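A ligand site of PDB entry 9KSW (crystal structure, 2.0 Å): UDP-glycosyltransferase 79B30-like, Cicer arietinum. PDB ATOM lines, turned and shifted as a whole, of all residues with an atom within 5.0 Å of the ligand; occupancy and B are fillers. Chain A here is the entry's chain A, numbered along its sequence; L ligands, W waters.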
ATOM      1  N   TRP A  14       6.873  18.162  11.318  1.00  0.00           N
ATOM      2  CA  TRP A  14       7.698  19.036  10.484  1.00  0.00           C
ATOM      3  C   TRP A  14       7.269  20.488  10.639  1.00  0.00           C
ATOM      4  O   TRP A  14       6.088  20.787  10.905  1.00  0.00           O
ATOM      5  CB  TRP A  14       7.580  18.558   9.021  1.00  0.00           C
ATOM      6  CG  TRP A  14       7.998  19.451   7.892  1.00  0.00           C
ATOM      7  CD1 TRP A  14       7.232  19.762   6.790  1.00  0.00           C
ATOM      8  CD2 TRP A  14       9.286  20.068   7.663  1.00  0.00           C
ATOM      9  NE1 TRP A  14       7.964  20.544   5.906  1.00  0.00           N
ATOM     10  CE2 TRP A  14       9.215  20.759   6.416  1.00  0.00           C
ATOM     11  CE3 TRP A  14      10.486  20.138   8.399  1.00  0.00           C
ATOM     12  CZ2 TRP A  14      10.294  21.502   5.888  1.00  0.00           C
ATOM     13  CZ3 TRP A  14      11.570  20.873   7.875  1.00  0.00           C
ATOM     14  CH2 TRP A  14      11.456  21.547   6.627  1.00  0.00           C
ATOM     15  N   ALA A  16       5.971  23.125   9.463  1.00  0.00           N
ATOM     16  CA  ALA A  16       5.124  23.639   8.390  1.00  0.00           C
ATOM     17  C   ALA A  16       3.684  23.651   8.859  1.00  0.00           C
ATOM     18  O   ALA A  16       3.257  22.764   9.596  1.00  0.00           O
ATOM     19  CB  ALA A  16       5.237  22.789   7.103  1.00  0.00           C
ATOM     20  N   HIS A  19       1.586  20.578   8.351  1.00  0.00           N
ATOM     21  CA  HIS A  19       1.756  19.482   9.294  1.00  0.00           C
ATOM     22  C   HIS A  19       1.295  19.827  10.704  1.00  0.00           C
ATOM     23  O   HIS A  19       0.707  18.976  11.391  1.00  0.00           O
ATOM     24  CB  HIS A  19       3.217  19.019   9.319  1.00  0.00           C
ATOM     25  CG  HIS A  19       3.673  18.445   8.007  1.00  0.00           C
ATOM     26  ND1 HIS A  19       4.211  17.182   7.887  1.00  0.00           N
ATOM     27  CD2 HIS A  19       3.641  18.966   6.748  1.00  0.00           C
ATOM     28  CE1 HIS A  19       4.502  16.949   6.615  1.00  0.00           C
ATOM     29  NE2 HIS A  19       4.172  18.019   5.908  1.00  0.00           N
ATOM     30  N   THR A  79       7.967  26.621   7.014  1.00  0.00           N
ATOM     31  CA  THR A  79       8.038  26.850   5.572  1.00  0.00           C
ATOM     32  C   THR A  79       7.223  28.052   5.131  1.00  0.00           C
ATOM     33  O   THR A  79       7.325  28.451   3.964  1.00  0.00           O
ATOM     34  CB  THR A  79       7.558  25.630   4.762  1.00  0.00           C
ATOM     35  OG1 THR A  79       6.223  25.278   5.178  1.00  0.00           O
ATOM     36  CG2 THR A  79       8.511  24.431   4.908  1.00  0.00           C
ATOM     37  N   ILE A  84      10.634  28.192  -1.086  1.00  0.00           N
ATOM     38  CA  ILE A  84      10.639  26.732  -1.194  1.00  0.00           C
ATOM     39  C   ILE A  84      12.048  26.231  -1.427  1.00  0.00           C
ATOM     40  O   ILE A  84      12.395  25.114  -1.005  1.00  0.00           O
ATOM     41  CB  ILE A  84       9.657  26.296  -2.306  1.00  0.00           C
ATOM     42  CG1 ILE A  84       9.734  24.783  -2.590  1.00  0.00           C
ATOM     43  CG2 ILE A  84       9.881  27.088  -3.587  1.00  0.00           C
ATOM     44  CD1 ILE A  84       9.089  23.897  -1.503  1.00  0.00           C
ATOM     45  N   PHE A 115       6.348  11.496  14.681  1.00  0.00           N
ATOM     46  CA  PHE A 115       7.330  12.425  14.100  1.00  0.00           C
ATOM     47  C   PHE A 115       7.287  12.433  12.576  1.00  0.00           C
ATOM     48  O   PHE A 115       6.764  11.513  11.938  1.00  0.00           O
ATOM     49  CB  PHE A 115       8.759  12.098  14.581  1.00  0.00           C
ATOM     50  CG  PHE A 115       9.320  10.841  13.982  1.00  0.00           C
ATOM     51  CD1 PHE A 115       8.898   9.588  14.432  1.00  0.00           C
ATOM     52  CD2 PHE A 115      10.253  10.894  12.952  1.00  0.00           C
ATOM     53  CE1 PHE A 115       9.401   8.424  13.854  1.00  0.00           C
ATOM     54  CE2 PHE A 115      10.776   9.744  12.398  1.00  0.00           C
ATOM     55  CZ  PHE A 115      10.343   8.499  12.851  1.00  0.00           C
ATOM     56  N   ASP A 116       7.871  13.491  11.992  1.00  0.00           N
ATOM     57  CA  ASP A 116       8.243  13.603  10.572  1.00  0.00           C
ATOM     58  C   ASP A 116       9.765  13.641  10.392  1.00  0.00           C
ATOM     59  O   ASP A 116      10.469  14.260  11.199  1.00  0.00           O
ATOM     60  CB  ASP A 116       7.731  14.904   9.944  1.00  0.00           C
ATOM     61  CG  ASP A 116       6.239  14.884   9.635  1.00  0.00           C
ATOM     62  OD1 ASP A 116       5.738  13.887   9.071  1.00  0.00           O
ATOM     63  OD2 ASP A 116       5.598  15.905   9.947  1.00  0.00           O
ATOM     64  N   PHE A 117      10.235  13.043   9.297  1.00  0.00           N
ATOM     65  CA  PHE A 117      11.535  13.380   8.691  1.00  0.00           C
ATOM     66  C   PHE A 117      12.808  13.045   9.479  1.00  0.00           C
ATOM     67  O   PHE A 117      13.830  12.757   8.866  1.00  0.00           O
ATOM     68  CB  PHE A 117      11.577  14.888   8.366  1.00  0.00           C
ATOM     69  CG  PHE A 117      10.903  15.242   7.066  1.00  0.00           C
ATOM     70  CD1 PHE A 117      11.150  14.521   5.912  1.00  0.00           C
ATOM     71  CD2 PHE A 117      10.026  16.317   7.010  1.00  0.00           C
ATOM     72  CE1 PHE A 117      10.542  14.866   4.705  1.00  0.00           C
ATOM     73  CE2 PHE A 117       9.399  16.650   5.805  1.00  0.00           C
ATOM     74  CZ  PHE A 117       9.663  15.921   4.662  1.00  0.00           C
ATOM     75  N   LEU A 134       6.309   7.000  12.886  1.00  0.00           N
ATOM     76  CA  LEU A 134       6.429   7.920  11.760  1.00  0.00           C
ATOM     77  C   LEU A 134       5.023   8.198  11.241  1.00  0.00           C
ATOM     78  O   LEU A 134       4.382   7.301  10.667  1.00  0.00           O
ATOM     79  CB  LEU A 134       7.329   7.312  10.698  1.00  0.00           C
ATOM     80  CG  LEU A 134       7.571   8.071   9.385  1.00  0.00           C
ATOM     81  CD1 LEU A 134       8.372   9.330   9.607  1.00  0.00           C
ATOM     82  CD2 LEU A 134       8.265   7.155   8.383  1.00  0.00           C
ATOM     83  N   PHE A 136       2.572  10.233   8.825  1.00  0.00           N
ATOM     84  CA  PHE A 136       2.405  11.058   7.619  1.00  0.00           C
ATOM     85  C   PHE A 136       1.004  11.652   7.519  1.00  0.00           C
ATOM     86  O   PHE A 136       0.015  10.931   7.610  1.00  0.00           O
ATOM     87  CB  PHE A 136       2.627  10.241   6.352  1.00  0.00           C
ATOM     88  CG  PHE A 136       3.974   9.631   6.213  1.00  0.00           C
ATOM     89  CD1 PHE A 136       5.007  10.345   5.598  1.00  0.00           C
ATOM     90  CD2 PHE A 136       4.207   8.320   6.645  1.00  0.00           C
ATOM     91  CE1 PHE A 136       6.258   9.760   5.452  1.00  0.00           C
ATOM     92  CE2 PHE A 136       5.442   7.750   6.499  1.00  0.00           C
ATOM     93  CZ  PHE A 136       6.470   8.466   5.892  1.00  0.00           C
ATOM     94  N   ILE A 138       0.431  13.195   4.540  1.00  0.00           N
ATOM     95  CA  ILE A 138       0.322  13.172   3.085  1.00  0.00           C
ATOM     96  C   ILE A 138      -0.204  11.801   2.673  1.00  0.00           C
ATOM     97  O   ILE A 138      -0.401  10.925   3.524  1.00  0.00           O
ATOM     98  CB  ILE A 138       1.669  13.477   2.392  1.00  0.00           C
ATOM     99  CG1 ILE A 138       2.708  12.386   2.714  1.00  0.00           C
ATOM    100  CG2 ILE A 138       2.145  14.877   2.731  1.00  0.00           C
ATOM    101  CD1 ILE A 138       3.893  12.350   1.718  1.00  0.00           C
ATOM    102  N   THR A 142       1.539   8.337  -2.334  1.00  0.00           N
ATOM    103  CA  THR A 142       2.737   9.069  -2.722  1.00  0.00           C
ATOM    104  C   THR A 142       4.003   8.375  -2.240  1.00  0.00           C
ATOM    105  O   THR A 142       4.916   8.081  -3.034  1.00  0.00           O
ATOM    106  CB  THR A 142       2.682  10.516  -2.186  1.00  0.00           C
ATOM    107  OG1 THR A 142       1.562  11.182  -2.748  1.00  0.00           O
ATOM    108  CG2 THR A 142       3.939  11.312  -2.579  1.00  0.00           C
ATOM    109  N   ILE A 143       4.062   8.082  -0.921  1.00  0.00           N
ATOM    110  CA  ILE A 143       5.177   7.317  -0.362  1.00  0.00           C
ATOM    111  C   ILE A 143       5.319   5.970  -1.082  1.00  0.00           C
ATOM    112  O   ILE A 143       6.438   5.527  -1.358  1.00  0.00           O
ATOM    113  CB  ILE A 143       4.966   7.114   1.153  1.00  0.00           C
ATOM    114  CG1 ILE A 143       5.026   8.447   1.888  1.00  0.00           C
ATOM    115  CG2 ILE A 143       6.025   6.150   1.737  1.00  0.00           C
ATOM    116  CD1 ILE A 143       6.334   9.172   1.731  1.00  0.00           C
ATOM    117  N   THR A 146       7.040   6.480  -4.677  1.00  0.00           N
ATOM    118  CA  THR A 146       8.388   7.027  -4.773  1.00  0.00           C
ATOM    119  C   THR A 146       9.416   6.393  -3.842  1.00  0.00           C
ATOM    120  O   THR A 146      10.622   6.488  -4.129  1.00  0.00           O
ATOM    121  CB  THR A 146       8.362   8.529  -4.478  1.00  0.00           C
ATOM    122  OG1 THR A 146       7.830   8.720  -3.155  1.00  0.00           O
ATOM    123  CG2 THR A 146       7.490   9.278  -5.465  1.00  0.00           C
ATOM    124  N   THR A 147       8.999   5.782  -2.736  1.00  0.00           N
ATOM    125  CA  THR A 147       9.901   5.442  -1.637  1.00  0.00           C
ATOM    126  C   THR A 147       9.742   3.990  -1.168  1.00  0.00           C
ATOM    127  O   THR A 147      10.254   3.641  -0.085  1.00  0.00           O
ATOM    128  CB  THR A 147       9.672   6.419  -0.456  1.00  0.00           C
ATOM    129  OG1 THR A 147       9.420   7.734  -0.974  1.00  0.00           O
ATOM    130  CG2 THR A 147      10.864   6.473   0.494  1.00  0.00           C
ATOM    131  N   HIS A 183      10.028  16.112 -12.752  1.00  0.00           N
ATOM    132  CA  HIS A 183      10.065  16.677 -11.414  1.00  0.00           C
ATOM    133  C   HIS A 183      10.435  15.628 -10.370  1.00  0.00           C
ATOM    134  O   HIS A 183      11.349  15.832  -9.575  1.00  0.00           O
ATOM    135  CB  HIS A 183       8.709  17.313 -11.080  1.00  0.00           C
ATOM    136  CG  HIS A 183       8.714  18.071  -9.788  1.00  0.00           C
ATOM    137  ND1 HIS A 183       9.443  19.228  -9.611  1.00  0.00           N
ATOM    138  CD2 HIS A 183       8.100  17.829  -8.606  1.00  0.00           C
ATOM    139  CE1 HIS A 183       9.262  19.675  -8.379  1.00  0.00           C
ATOM    140  NE2 HIS A 183       8.454  18.845  -7.744  1.00  0.00           N
ATOM    141  N   LEU A 184       9.730  14.495 -10.352  1.00  0.00           N
ATOM    142  CA  LEU A 184      10.001  13.454  -9.363  1.00  0.00           C
ATOM    143  C   LEU A 184      11.441  12.937  -9.452  1.00  0.00           C
ATOM    144  O   LEU A 184      12.080  12.649  -8.438  1.00  0.00           O
ATOM    145  CB  LEU A 184       9.027  12.290  -9.518  1.00  0.00           C
ATOM    146  CG  LEU A 184       7.572  12.536  -9.090  1.00  0.00           C
ATOM    147  CD1 LEU A 184       6.730  11.273  -9.339  1.00  0.00           C
ATOM    148  CD2 LEU A 184       7.514  12.948  -7.626  1.00  0.00           C
ATOM    149  N   THR A 187      13.947  16.008  -8.205  1.00  0.00           N
ATOM    150  CA  THR A 187      13.835  16.471  -6.819  1.00  0.00           C
ATOM    151  C   THR A 187      14.183  15.387  -5.810  1.00  0.00           C
ATOM    152  O   THR A 187      14.652  15.707  -4.708  1.00  0.00           O
ATOM    153  CB  THR A 187      12.433  17.024  -6.528  1.00  0.00           C
ATOM    154  OG1 THR A 187      11.433  16.025  -6.831  1.00  0.00           O
ATOM    155  CG2 THR A 187      12.181  18.301  -7.343  1.00  0.00           C
ATOM    156  N   ARG A 188      13.983  14.115  -6.139  1.00  0.00           N
ATOM    157  CA  ARG A 188      14.231  13.032  -5.171  1.00  0.00           C
ATOM    158  C   ARG A 188      15.688  12.933  -4.773  1.00  0.00           C
ATOM    159  O   ARG A 188      15.986  12.430  -3.679  1.00  0.00           O
ATOM    160  CB  ARG A 188      13.773  11.682  -5.721  1.00  0.00           C
ATOM    161  CG  ARG A 188      14.709  11.078  -6.773  1.00  0.00           C
ATOM    162  CD  ARG A 188      14.106   9.799  -7.355  1.00  0.00           C
ATOM    163  NE  ARG A 188      14.241   8.692  -6.411  1.00  0.00           N
ATOM    164  CZ  ARG A 188      13.230   8.081  -5.807  1.00  0.00           C
ATOM    165  NH1 ARG A 188      11.983   8.462  -5.993  1.00  0.00           N
ATOM    166  NH2 ARG A 188      13.479   7.040  -5.001  1.00  0.00           N
ATOM    167  N   PHE A 192      17.989  17.342   1.218  1.00  0.00           N
ATOM    168  CA  PHE A 192      16.956  17.958   2.059  1.00  0.00           C
ATOM    169  C   PHE A 192      17.438  17.840   3.503  1.00  0.00           C
ATOM    170  O   PHE A 192      17.043  16.935   4.240  1.00  0.00           O
ATOM    171  CB  PHE A 192      15.580  17.269   1.853  1.00  0.00           C
ATOM    172  CG  PHE A 192      14.420  17.988   2.512  1.00  0.00           C
ATOM    173  CD1 PHE A 192      13.961  19.207   2.027  1.00  0.00           C
ATOM    174  CD2 PHE A 192      13.769  17.424   3.602  1.00  0.00           C
ATOM    175  CE1 PHE A 192      12.898  19.869   2.612  1.00  0.00           C
ATOM    176  CE2 PHE A 192      12.687  18.061   4.215  1.00  0.00           C
ATOM    177  CZ  PHE A 192      12.253  19.304   3.718  1.00  0.00           C
ATOM    178  N   PHE A 198      16.629  13.729  -0.600  1.00  0.00           N
ATOM    179  CA  PHE A 198      15.247  13.735  -0.116  1.00  0.00           C
ATOM    180  C   PHE A 198      14.668  12.338   0.020  1.00  0.00           C
ATOM    181  O   PHE A 198      14.122  11.995   1.066  1.00  0.00           O
ATOM    182  CB  PHE A 198      14.342  14.579  -1.017  1.00  0.00           C
ATOM    183  CG  PHE A 198      12.909  14.693  -0.496  1.00  0.00           C
ATOM    184  CD1 PHE A 198      12.607  15.508   0.585  1.00  0.00           C
ATOM    185  CD2 PHE A 198      11.884  13.958  -1.079  1.00  0.00           C
ATOM    186  CE1 PHE A 198      11.283  15.616   1.082  1.00  0.00           C
ATOM    187  CE2 PHE A 198      10.554  14.060  -0.585  1.00  0.00           C
ATOM    188  CZ  PHE A 198      10.270  14.887   0.495  1.00  0.00           C
ATOM    189  N   SER A 199      14.731  11.516  -1.026  1.00  0.00           N
ATOM    190  CA  SER A 199      14.065  10.222  -0.865  1.00  0.00           C
ATOM    191  C   SER A 199      14.812   9.299   0.087  1.00  0.00           C
ATOM    192  O   SER A 199      14.184   8.458   0.745  1.00  0.00           O
ATOM    193  CB  SER A 199      13.832   9.577  -2.225  1.00  0.00           C
ATOM    194  OG  SER A 199      12.755  10.233  -2.878  1.00  0.00           O
ATOM    195  N   SER A 202      13.404   9.768   4.690  1.00  0.00           N
ATOM    196  CA  SER A 202      12.089   9.175   4.416  1.00  0.00           C
ATOM    197  C   SER A 202      12.253   7.665   4.358  1.00  0.00           C
ATOM    198  O   SER A 202      11.690   6.955   5.187  1.00  0.00           O
ATOM    199  CB  SER A 202      11.393   9.639   3.123  1.00  0.00           C
ATOM    200  OG  SER A 202      10.763  10.905   3.266  1.00  0.00           O
ATOM    201  N   CYS A 205      13.677   6.909   7.497  1.00  0.00           N
ATOM    202  CA  CYS A 205      12.613   6.996   8.482  1.00  0.00           C
ATOM    203  C   CYS A 205      11.734   5.764   8.446  1.00  0.00           C
ATOM    204  O   CYS A 205      11.389   5.192   9.486  1.00  0.00           O
ATOM    205  CB  CYS A 205      11.756   8.236   8.249  1.00  0.00           C
ATOM    206  SG  CYS A 205      12.542   9.817   8.600  1.00  0.00           S
ATOM    207  N   GLU A 275       3.117  27.844   0.499  1.00  0.00           N
ATOM    208  CA  GLU A 275       4.493  27.412   0.284  1.00  0.00           C
ATOM    209  C   GLU A 275       5.059  27.799  -1.080  1.00  0.00           C
ATOM    210  O   GLU A 275       6.228  27.442  -1.358  1.00  0.00           O
ATOM    211  CB  GLU A 275       4.614  25.878   0.466  1.00  0.00           C
ATOM    212  CG  GLU A 275       4.565  25.368   1.911  1.00  0.00           C
ATOM    213  CD  GLU A 275       5.277  24.027   2.097  1.00  0.00           C
ATOM    214  OE1 GLU A 275       5.697  23.430   1.066  1.00  0.00           O
ATOM    215  OE2 GLU A 275       5.442  23.571   3.267  1.00  0.00           O
ATOM    216  N   LEU A 372       3.807  21.889  -8.523  1.00  0.00           N
ATOM    217  CA  LEU A 372       4.880  20.913  -8.736  1.00  0.00           C
ATOM    218  C   LEU A 372       5.346  20.355  -7.403  1.00  0.00           C
ATOM    219  O   LEU A 372       6.262  20.878  -6.756  1.00  0.00           O
ATOM    220  CB  LEU A 372       6.027  21.541  -9.518  1.00  0.00           C
ATOM    221  CG  LEU A 372       6.047  21.435 -11.059  1.00  0.00           C
ATOM    222  CD1 LEU A 372       7.334  22.017 -11.646  1.00  0.00           C
ATOM    223  CD2 LEU A 372       5.809  20.020 -11.588  1.00  0.00           C
ATOM    224  N   ASN A 373       4.762  19.237  -7.017  1.00  0.00           N
ATOM    225  CA  ASN A 373       5.060  18.543  -5.765  1.00  0.00           C
ATOM    226  C   ASN A 373       4.474  17.152  -5.913  1.00  0.00           C
ATOM    227  O   ASN A 373       3.375  16.999  -6.426  1.00  0.00           O
ATOM    228  CB  ASN A 373       4.477  19.311  -4.550  1.00  0.00           C
ATOM    229  CG  ASN A 373       4.436  18.485  -3.264  1.00  0.00           C
ATOM    230  OD1 ASN A 373       3.730  17.484  -3.179  1.00  0.00           O
ATOM    231  ND2 ASN A 373       5.194  18.911  -2.251  1.00  0.00           N
ATOM    232  N   GLY A 374       5.238  16.132  -5.492  1.00  0.00           N
ATOM    233  CA  GLY A 374       4.808  14.754  -5.731  1.00  0.00           C
ATOM    234  C   GLY A 374       3.458  14.438  -5.099  1.00  0.00           C
ATOM    235  O   GLY A 374       2.582  13.847  -5.747  1.00  0.00           O
ATOM    236  N   ASP A 375       3.258  14.811  -3.833  1.00  0.00           N
ATOM    237  CA  ASP A 375       1.960  14.539  -3.209  1.00  0.00           C
ATOM    238  C   ASP A 375       0.840  15.296  -3.915  1.00  0.00           C
ATOM    239  O   ASP A 375      -0.243  14.745  -4.138  1.00  0.00           O
ATOM    240  CB  ASP A 375       1.972  14.895  -1.715  1.00  0.00           C
ATOM    241  CG  ASP A 375       0.802  14.219  -0.943  1.00  0.00           C
ATOM    242  OD1 ASP A 375       0.674  12.973  -1.035  1.00  0.00           O
ATOM    243  OD2 ASP A 375       0.012  14.920  -0.265  1.00  0.00           O
HETATM  244  O1  LIG L   1       7.314  13.128   1.263  1.00  0.00           O
HETATM  245  C1  LIG L   1       6.834  14.132   2.070  1.00  0.00           C
HETATM  246  C2  LIG L   1       6.231  15.276   1.511  1.00  0.00           C
HETATM  247  O2  LIG L   1       5.782  16.292   2.349  1.00  0.00           O
HETATM  248  C3  LIG L   1       6.126  15.378   0.126  1.00  0.00           C
HETATM  249  O3  LIG L   1       5.571  16.376  -0.419  1.00  0.00           O
HETATM  250  C4  LIG L   1       6.630  14.338  -2.132  1.00  0.00           C
HETATM  251  O4  LIG L   1       6.073  15.394  -2.782  1.00  0.00           O
HETATM  252  C5  LIG L   1       7.166  13.297  -2.861  1.00  0.00           C
HETATM  253  C6  LIG L   1       7.749  12.219  -2.190  1.00  0.00           C
HETATM  254  O5  LIG L   1       8.271  11.208  -2.920  1.00  0.00           O
HETATM  255  C7  LIG L   1       7.793  12.145  -0.800  1.00  0.00           C
HETATM  256  C8  LIG L   1       7.253  13.206  -0.101  1.00  0.00           C
HETATM  257  C9  LIG L   1       6.668  14.316  -0.716  1.00  0.00           C
HETATM  258  C10 LIG L   1       7.016  13.824   3.497  1.00  0.00           C
HETATM  259  C11 LIG L   1       8.039  12.945   3.877  1.00  0.00           C
HETATM  260  C12 LIG L   1       8.245  12.622   5.201  1.00  0.00           C
HETATM  261  O6  LIG L   1       9.273  11.784   5.579  1.00  0.00           O
HETATM  262  C13 LIG L   1       7.418  13.167   6.187  1.00  0.00           C
HETATM  263  O7  LIG L   1       7.676  12.800   7.467  1.00  0.00           O
HETATM  264  C14 LIG L   1       6.399  14.027   5.836  1.00  0.00           C
HETATM  265  C15 LIG L   1       6.186  14.350   4.496  1.00  0.00           C
HETATM  266  C16 LIG L   1       6.088  17.633   1.955  1.00  0.00           C
HETATM  267  C17 LIG L   1       5.795  18.627   3.080  1.00  0.00           C
HETATM  268  O8  LIG L   1       4.393  18.652   3.343  1.00  0.00           O
HETATM  269  C18 LIG L   1       6.229  20.030   2.642  1.00  0.00           C
HETATM  270  O9  LIG L   1       6.078  20.956   3.713  1.00  0.00           O
HETATM  271  C19 LIG L   1       7.660  20.058   2.114  1.00  0.00           C
HETATM  272  O10 LIG L   1       7.940  21.351   1.601  1.00  0.00           O
HETATM  273  C20 LIG L   1       7.778  19.005   1.002  1.00  0.00           C
HETATM  274  C21 LIG L   1       9.134  18.913   0.355  1.00  0.00           C
HETATM  275  O11 LIG L   1       7.445  17.704   1.541  1.00  0.00           O
HETATM  276  C22 LIG L   1      10.130  17.832  -1.560  1.00  0.00           C
HETATM  277  O12 LIG L   1       8.983  18.064  -0.805  1.00  0.00           O
HETATM  278  C23 LIG L   1       9.745  16.916  -2.721  1.00  0.00           C
HETATM  279  O13 LIG L   1      10.899  16.478  -3.444  1.00  0.00           O
HETATM  280  C24 LIG L   1       8.803  17.654  -3.669  1.00  0.00           C
HETATM  281  O14 LIG L   1       8.435  16.831  -4.782  1.00  0.00           O
HETATM  282  C25 LIG L   1       9.438  18.947  -4.139  1.00  0.00           C
HETATM  283  O15 LIG L   1       8.514  19.656  -4.951  1.00  0.00           O
HETATM  284  C26 LIG L   1       9.828  19.787  -2.929  1.00  0.00           C
HETATM  285  C27 LIG L   1      10.567  21.046  -3.303  1.00  0.00           C
HETATM  286  O16 LIG L   1      10.686  19.041  -2.035  1.00  0.00           O
HETATM  287  O   HOH W   1      10.261  11.929  -4.579  1.00  0.00           O
HETATM  288  O   HOH W   2      10.666  14.379  -4.942  1.00  0.00           O
HETATM  289  O   HOH W   3       3.100  21.450   4.212  1.00  0.00           O
HETATM  290  O   HOH W   4      13.266  20.458  -1.285  1.00  0.00           O
HETATM  291  O   HOH W   5      10.104  22.681   2.161  1.00  0.00           O
HETATM  292  O   HOH W   6      13.493  17.838  -3.038  1.00  0.00           O
HETATM  293  O   HOH W   7       2.333  19.574   1.511  1.00  0.00           O
HETATM  294  O   HOH W   8      10.536  10.352  -1.540  1.00  0.00           O
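CB of Ala 16 touches O9 of the ligand (3.9 Å).
Ile 84 touches the ligand.
CE1 of Phe 136 touches C12 of the ligand, 3.5 Å away.
Ile 138 touches the ligand.
Thr 142 touches the ligand (CG2 to C5, 3.8 Å).
Phe 198 touches the ligand (CE2 to C7, 3.4 Å).
Of the 29 residues printed, 19 come within 4 Å of the ligand.
The backbone carbonyl oxygen of His 183 is in hydrogen-bond range of the side-chain hydroxyl of Thr 187.
The backbone carbonyl oxygen (O) of Phe 117 is in hydrogen-bond range of the side-chain sulfur (SG) of Cys 205, 3.2 Å away.
N of Asp 375 sits at hydrogen-bond distance from OD1 of Asn 373, at 2.8 Å.
The side-chain carboxylate (OD1) of Asp 375 lies within hydrogen-bond range of the side-chain hydroxyl (OG1) of Thr 142 (2.6 Å).
A ring nitrogen (NE2) of His 183 is in hydrogen-bond range of the backbone carbonyl oxygen of Leu 372 (3.1 Å).
O of Thr 146 sits at hydrogen-bond distance from NH2 of Arg 188 (3.0 Å).
The side-chain hydroxyl of Thr 146 sits at hydrogen-bond distance from the side-chain hydroxyl of Thr 147.
N of Trp 14 is in hydrogen-bond range of OD2 of Asp 116, at 2.9 Å.
An oxygen (O8) of the ligand lies within hydrogen-bond range of a ring nitrogen (NE2) of His 19.
The backbone NH (N) of Gly 374 lies within hydrogen-bond range of an oxygen (O4) of the ligand.
O9 of the ligand is in hydrogen-bond range of NE1 of Trp 14, at 2.9 Å.
An oxygen (O6) of the ligand is in hydrogen-bond range of the side-chain hydroxyl of Ser 202.
The backbone NH (N) of Phe 117 sits at hydrogen-bond distance from an oxygen (O7) of the ligand (3.2 Å).
The side-chain hydroxyl of Thr 146 is in hydrogen-bond range of an oxygen (O5) of the ligand.
The side-chain hydroxyl (OG1) of Thr 187 is in hydrogen-bond range of an oxygen (O13) of the ligand, 3.5 Å away.
The side-chain carboxylate of Asp 116 is in hydrogen-bond range of an oxygen (O7) of the ligand (2.7 Å).
A ring nitrogen (NE2) of His 183 lies within hydrogen-bond range of an oxygen (O15) of the ligand.
ND2 of Asn 373 sits at hydrogen-bond distance from O3 of the ligand (3.2 Å).
An oxygen (O15) of the ligand sits at hydrogen-bond distance from the backbone carbonyl oxygen of Leu 372 (3.1 Å).
The backbone NH (N) of Asp 375 is in hydrogen-bond range of an oxygen (O4) of the ligand (3.1 Å).
The side-chain carboxylate of Glu 275 lies within hydrogen-bond range of an oxygen (O9) of the ligand (2.7 Å).
Water W2 lies within hydrogen-bond range of O13 of the ligand (2.6 Å) and OG1 of Thr 187 (2.6 Å).
Water W1 bridges O5 of the ligand (2.7 Å) and OG of Ser 199 (3.5 Å).
Water W8 lies within hydrogen-bond range of OG of Ser 199, O5 of the ligand and OG1 of Thr 147.
Water W6 lies within hydrogen-bond range of O of Thr 187 (2.9 Å) and O13 of the ligand (3.0 Å).
Water W3 bridges an oxygen (O9) of the ligand and the side-chain carboxylate (OE2) of Glu 275.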
